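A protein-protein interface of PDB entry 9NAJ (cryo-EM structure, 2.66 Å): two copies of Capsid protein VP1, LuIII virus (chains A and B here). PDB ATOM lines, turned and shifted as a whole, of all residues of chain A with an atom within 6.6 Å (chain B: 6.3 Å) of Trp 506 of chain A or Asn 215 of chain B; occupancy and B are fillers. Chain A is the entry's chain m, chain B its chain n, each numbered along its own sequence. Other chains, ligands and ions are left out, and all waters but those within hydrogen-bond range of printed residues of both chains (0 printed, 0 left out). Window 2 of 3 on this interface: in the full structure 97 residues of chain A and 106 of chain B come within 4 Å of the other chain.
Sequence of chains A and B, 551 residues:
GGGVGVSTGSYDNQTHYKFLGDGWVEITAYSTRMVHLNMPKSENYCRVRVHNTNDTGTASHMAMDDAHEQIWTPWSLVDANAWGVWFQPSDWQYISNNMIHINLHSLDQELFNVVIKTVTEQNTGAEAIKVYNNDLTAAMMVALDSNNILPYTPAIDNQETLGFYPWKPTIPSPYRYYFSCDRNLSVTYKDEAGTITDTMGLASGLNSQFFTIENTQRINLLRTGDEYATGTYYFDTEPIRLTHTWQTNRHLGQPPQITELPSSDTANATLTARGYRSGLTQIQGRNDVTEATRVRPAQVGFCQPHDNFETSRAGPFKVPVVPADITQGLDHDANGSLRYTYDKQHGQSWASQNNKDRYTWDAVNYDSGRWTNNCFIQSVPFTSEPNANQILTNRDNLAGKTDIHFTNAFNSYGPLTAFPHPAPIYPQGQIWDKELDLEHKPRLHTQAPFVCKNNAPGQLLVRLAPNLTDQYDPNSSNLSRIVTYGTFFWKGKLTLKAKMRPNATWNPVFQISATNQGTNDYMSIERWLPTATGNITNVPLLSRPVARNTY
N of Trp 506 of chain A lies within hydrogen-bond range of O of Phe 210 of chain B.
ND2 of Asn 507 of chain A lies close to N of Phe 210 of chain B (3.2 Å).
OG1 of Thr 216 of chain B sits at hydrogen-bond distance from O of Thr 212 of chain B (2.7 Å).
The backbone carbonyl oxygen of Ile 213 of chain B sits at hydrogen-bond distance from the side-chain hydroxyl of Thr 216 of chain B (3.5 Å).
Among the printed residues, pairs that only touch across the chains: Ala 504 of chain A with Phe 211 of chain B (3.8 Å), Ala 504 of chain A with Thr 216 of chain B (3.5 Å), Thr 505 of chain A with Phe 210 of chain B (3.2 Å), Thr 505 of chain A with Phe 211 of chain B (3.5 Å) and Trp 506 of chain A with Asn 215 of chain B (3.6 Å).
Printed residues of chain B that touch a printed residue of chain A: Phe 210, Phe 211, Asn 215 and Thr 216.
Hydrophobic or aromatic side chains of chain B within 4 Å of the printed part of chain A: Phe 210 and Phe 211.
Printed residues of chain A that touch a printed residue of chain B: Ala 504, Thr 505, Trp 506 and Asn 507.
Hydrophobic or aromatic side chains of chain A within 4 Å of the printed part of chain B: Ala 504 and Trp 506.
Along chain A the printed residues that touch a printed residue of chain B span positions 504 to 507.
Among the printed residues, 7 pairs touch across the chains.
Among the printed residues, no Asp or Glu carboxylate lies within 4 Å of a Lys or Arg side-chain nitrogen of the other chain.
No position is printed for both chains.
Of the 7 pairs that touch across the chains among the printed residues, none has its exchanged pair printed and touching as well.
Of the printed residues of chain B, Thr 505 of chain A touches Phe 210 (3.2 Å) and Phe 211 (3.5 Å).
Trp 506 of chain A touches just these residues of chain B: Phe 210 (2.9 Å) and Asn 215 (3.6 Å).
Of the printed residues of chain A, Phe 211 of chain B touches Ala 504 (3.8 Å) and Thr 505 (3.5 Å).
Ile 213 of chain B touches none of the printed residues of chain A.
Asn 215 of chain B touches one residue of chain A.
Of the printed residues of chain A, Thr 216 of chain B touches Ala 504 (3.5 Å).
Gln 217 of chain B touches none of the printed residues of chain A.
The nearest residue of chain B that does not touch Trp 506 of chain A is Thr 212 of chain B (4.4 Å).
The nearest printed residue of chain A that does not touch Phe 211 of chain B is Trp 506 of chain A (4.9 Å).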
ATOM      1  N   ALA A 504     -14.175  -6.227  16.032  1.00  0.00           N
ATOM      2  CA  ALA A 504     -13.123  -5.366  15.528  1.00  0.00           C
ATOM      3  C   ALA A 504     -12.062  -6.101  14.730  1.00  0.00           C
ATOM      4  O   ALA A 504     -11.161  -5.457  14.191  1.00  0.00           O
ATOM      5  CB  ALA A 504     -12.459  -4.635  16.687  1.00  0.00           C
ATOM      6  N   THR A 505     -12.134  -7.416  14.645  1.00  0.00           N
ATOM      7  CA  THR A 505     -11.031  -8.169  14.080  1.00  0.00           C
ATOM      8  C   THR A 505     -11.139  -8.215  12.565  1.00  0.00           C
ATOM      9  O   THR A 505     -12.232  -8.213  12.003  1.00  0.00           O
ATOM     10  CB  THR A 505     -11.008  -9.576  14.666  1.00  0.00           C
ATOM     11  OG1 THR A 505     -10.881  -9.486  16.085  1.00  0.00           O
ATOM     12  CG2 THR A 505      -9.825 -10.323  14.168  1.00  0.00           C
ATOM     13  N   TRP A 506      -9.987  -8.218  11.902  1.00  0.00           N
ATOM     14  CA  TRP A 506      -9.972  -8.428  10.461  1.00  0.00           C
ATOM     15  C   TRP A 506     -10.468  -9.818  10.109  1.00  0.00           C
ATOM     16  O   TRP A 506     -11.303  -9.988   9.218  1.00  0.00           O
ATOM     17  CB  TRP A 506      -8.563  -8.235   9.918  1.00  0.00           C
ATOM     18  CG  TRP A 506      -8.445  -8.515   8.465  1.00  0.00           C
ATOM     19  CD1 TRP A 506      -7.995  -9.656   7.897  1.00  0.00           C
ATOM     20  CD2 TRP A 506      -8.719  -7.617   7.398  1.00  0.00           C
ATOM     21  NE1 TRP A 506      -8.009  -9.546   6.538  1.00  0.00           N
ATOM     22  CE2 TRP A 506      -8.447  -8.297   6.205  1.00  0.00           C
ATOM     23  CE3 TRP A 506      -9.186  -6.309   7.333  1.00  0.00           C
ATOM     24  CZ2 TRP A 506      -8.623  -7.716   4.966  1.00  0.00           C
ATOM     25  CZ3 TRP A 506      -9.361  -5.737   6.104  1.00  0.00           C
ATOM     26  CH2 TRP A 506      -9.081  -6.435   4.936  1.00  0.00           C
ATOM     27  N   ASN A 507      -9.963 -10.825  10.799  1.00  0.00           N
ATOM     28  CA  ASN A 507     -10.194 -12.194  10.402  1.00  0.00           C
ATOM     29  C   ASN A 507     -11.537 -12.692  10.913  1.00  0.00           C
ATOM     30  O   ASN A 507     -12.110 -12.124  11.839  1.00  0.00           O
ATOM     31  CB  ASN A 507      -9.053 -13.069  10.909  1.00  0.00           C
ATOM     32  CG  ASN A 507      -8.970 -13.131  12.420  1.00  0.00           C
ATOM     33  OD1 ASN A 507      -9.969 -13.213  13.116  1.00  0.00           O
ATOM     34  ND2 ASN A 507      -7.765 -13.051  12.933  1.00  0.00           N
ATOM     35  N   PRO A 508     -12.071 -13.740  10.303  1.00  0.00           N
ATOM     36  CA  PRO A 508     -13.316 -14.319  10.798  1.00  0.00           C
ATOM     37  C   PRO A 508     -13.140 -15.001  12.143  1.00  0.00           C
ATOM     38  O   PRO A 508     -12.150 -15.686  12.390  1.00  0.00           O
ATOM     39  CB  PRO A 508     -13.682 -15.323   9.708  1.00  0.00           C
ATOM     40  CG  PRO A 508     -13.073 -14.768   8.500  1.00  0.00           C
ATOM     41  CD  PRO A 508     -11.776 -14.191   8.938  1.00  0.00           C
ATOM     42  N   TYR B  45       1.163  -5.012   7.621  1.00  0.00           N
ATOM     43  CA  TYR B  45       1.052  -5.791   8.839  1.00  0.00           C
ATOM     44  C   TYR B  45       1.703  -7.144   8.624  1.00  0.00           C
ATOM     45  O   TYR B  45       1.431  -7.829   7.640  1.00  0.00           O
ATOM     46  CB  TYR B  45      -0.406  -5.966   9.228  1.00  0.00           C
ATOM     47  CG  TYR B  45      -1.081  -4.687   9.620  1.00  0.00           C
ATOM     48  CD1 TYR B  45      -1.042  -4.241  10.921  1.00  0.00           C
ATOM     49  CD2 TYR B  45      -1.750  -3.925   8.690  1.00  0.00           C
ATOM     50  CE1 TYR B  45      -1.655  -3.081  11.286  1.00  0.00           C
ATOM     51  CE2 TYR B  45      -2.363  -2.761   9.048  1.00  0.00           C
ATOM     52  CZ  TYR B  45      -2.313  -2.342  10.349  1.00  0.00           C
ATOM     53  OH  TYR B  45      -2.926  -1.176  10.720  1.00  0.00           O
ATOM     54  N   PHE B 210      -6.490 -10.762  14.738  1.00  0.00           N
ATOM     55  CA  PHE B 210      -5.654  -9.840  13.987  1.00  0.00           C
ATOM     56  C   PHE B 210      -6.379  -8.514  13.848  1.00  0.00           C
ATOM     57  O   PHE B 210      -7.404  -8.425  13.171  1.00  0.00           O
ATOM     58  CB  PHE B 210      -5.273 -10.431  12.637  1.00  0.00           C
ATOM     59  CG  PHE B 210      -4.725  -9.433  11.683  1.00  0.00           C
ATOM     60  CD1 PHE B 210      -3.513  -8.836  11.903  1.00  0.00           C
ATOM     61  CD2 PHE B 210      -5.381  -9.174  10.508  1.00  0.00           C
ATOM     62  CE1 PHE B 210      -3.018  -7.926  11.012  1.00  0.00           C
ATOM     63  CE2 PHE B 210      -4.880  -8.282   9.609  1.00  0.00           C
ATOM     64  CZ  PHE B 210      -3.698  -7.657   9.860  1.00  0.00           C
ATOM     65  N   PHE B 211      -5.834  -7.490  14.483  1.00  0.00           N
ATOM     66  CA  PHE B 211      -6.409  -6.161  14.476  1.00  0.00           C
ATOM     67  C   PHE B 211      -5.610  -5.260  13.557  1.00  0.00           C
ATOM     68  O   PHE B 211      -4.398  -5.405  13.409  1.00  0.00           O
ATOM     69  CB  PHE B 211      -6.422  -5.553  15.871  1.00  0.00           C
ATOM     70  CG  PHE B 211      -7.253  -6.301  16.844  1.00  0.00           C
ATOM     71  CD1 PHE B 211      -8.610  -6.102  16.905  1.00  0.00           C
ATOM     72  CD2 PHE B 211      -6.673  -7.194  17.711  1.00  0.00           C
ATOM     73  CE1 PHE B 211      -9.371  -6.787  17.803  1.00  0.00           C
ATOM     74  CE2 PHE B 211      -7.431  -7.879  18.611  1.00  0.00           C
ATOM     75  CZ  PHE B 211      -8.781  -7.676  18.658  1.00  0.00           C
ATOM     76  N   THR B 212      -6.309  -4.331  12.940  1.00  0.00           N
ATOM     77  CA  THR B 212      -5.719  -3.337  12.069  1.00  0.00           C
ATOM     78  C   THR B 212      -6.032  -1.961  12.624  1.00  0.00           C
ATOM     79  O   THR B 212      -7.145  -1.712  13.085  1.00  0.00           O
ATOM     80  CB  THR B 212      -6.260  -3.486  10.658  1.00  0.00           C
ATOM     81  OG1 THR B 212      -5.845  -4.748  10.128  1.00  0.00           O
ATOM     82  CG2 THR B 212      -5.773  -2.396   9.780  1.00  0.00           C
ATOM     83  N   ILE B 213      -5.040  -1.077  12.610  1.00  0.00           N
ATOM     84  CA  ILE B 213      -5.275   0.273  13.098  1.00  0.00           C
ATOM     85  C   ILE B 213      -6.318   0.959  12.236  1.00  0.00           C
ATOM     86  O   ILE B 213      -7.245   1.598  12.740  1.00  0.00           O
ATOM     87  CB  ILE B 213      -3.964   1.069  13.116  1.00  0.00           C
ATOM     88  CG1 ILE B 213      -2.890   0.304  13.872  1.00  0.00           C
ATOM     89  CG2 ILE B 213      -4.185   2.401  13.764  1.00  0.00           C
ATOM     90  CD1 ILE B 213      -3.224   0.002  15.256  1.00  0.00           C
ATOM     91  N   GLU B 214      -6.192   0.818  10.920  1.00  0.00           N
ATOM     92  CA  GLU B 214      -7.083   1.502   9.997  1.00  0.00           C
ATOM     93  C   GLU B 214      -8.526   1.052  10.145  1.00  0.00           C
ATOM     94  O   GLU B 214      -9.440   1.863   9.986  1.00  0.00           O
ATOM     95  CB  GLU B 214      -6.595   1.281   8.572  1.00  0.00           C
ATOM     96  CG  GLU B 214      -5.293   1.991   8.261  1.00  0.00           C
ATOM     97  CD  GLU B 214      -4.072   1.264   8.780  1.00  0.00           C
ATOM     98  OE1 GLU B 214      -4.229   0.243   9.473  1.00  0.00           O
ATOM     99  OE2 GLU B 214      -2.946   1.716   8.494  1.00  0.00           O
ATOM    100  N   ASN B 215      -8.758  -0.219  10.421  1.00  0.00           N
ATOM    101  CA  ASN B 215     -10.122  -0.695  10.564  1.00  0.00           C
ATOM    102  C   ASN B 215     -10.733  -0.411  11.923  1.00  0.00           C
ATOM    103  O   ASN B 215     -11.957  -0.373  12.028  1.00  0.00           O
ATOM    104  CB  ASN B 215     -10.186  -2.185  10.275  1.00  0.00           C
ATOM    105  CG  ASN B 215     -10.025  -2.488   8.816  1.00  0.00           C
ATOM    106  OD1 ASN B 215     -10.948  -2.313   8.031  1.00  0.00           O
ATOM    107  ND2 ASN B 215      -8.846  -2.935   8.438  1.00  0.00           N
ATOM    108  N   THR B 216      -9.935  -0.279  12.971  1.00  0.00           N
ATOM    109  CA  THR B 216     -10.475  -0.074  14.302  1.00  0.00           C
ATOM    110  C   THR B 216     -10.497   1.365  14.789  1.00  0.00           C
ATOM    111  O   THR B 216     -11.032   1.612  15.870  1.00  0.00           O
ATOM    112  CB  THR B 216      -9.686  -0.905  15.316  1.00  0.00           C
ATOM    113  OG1 THR B 216      -8.313  -0.522  15.261  1.00  0.00           O
ATOM    114  CG2 THR B 216      -9.796  -2.361  14.980  1.00  0.00           C
ATOM    115  N   GLN B 217      -9.961   2.320  14.041  1.00  0.00           N
ATOM    116  CA  GLN B 217      -9.686   3.628  14.610  1.00  0.00           C
ATOM    117  C   GLN B 217     -10.113   4.720  13.649  1.00  0.00           C
ATOM    118  O   GLN B 217     -10.273   4.493  12.451  1.00  0.00           O
ATOM    119  CB  GLN B 217      -8.199   3.801  14.920  1.00  0.00           C
ATOM    120  CG  GLN B 217      -7.652   2.836  15.940  1.00  0.00           C
ATOM    121  CD  GLN B 217      -8.360   2.933  17.252  1.00  0.00           C
ATOM    122  OE1 GLN B 217      -8.701   4.018  17.703  1.00  0.00           O
ATOM    123  NE2 GLN B 217      -8.595   1.793  17.879  1.00  0.00           N
ATOM    124  N   ILE B 219      -8.476   7.935  12.151  1.00  0.00           N
ATOM    125  CA  ILE B 219      -7.146   8.497  11.988  1.00  0.00           C
ATOM    126  C   ILE B 219      -7.262   9.952  11.573  1.00  0.00           C
ATOM    127  O   ILE B 219      -8.004  10.284  10.644  1.00  0.00           O
ATOM    128  CB  ILE B 219      -6.326   7.695  10.968  1.00  0.00           C
ATOM    129  CG1 ILE B 219      -5.993   6.319  11.527  1.00  0.00           C
ATOM    130  CG2 ILE B 219      -5.060   8.414  10.629  1.00  0.00           C
ATOM    131  CD1 ILE B 219      -6.879   5.225  11.052  1.00  0.00           C
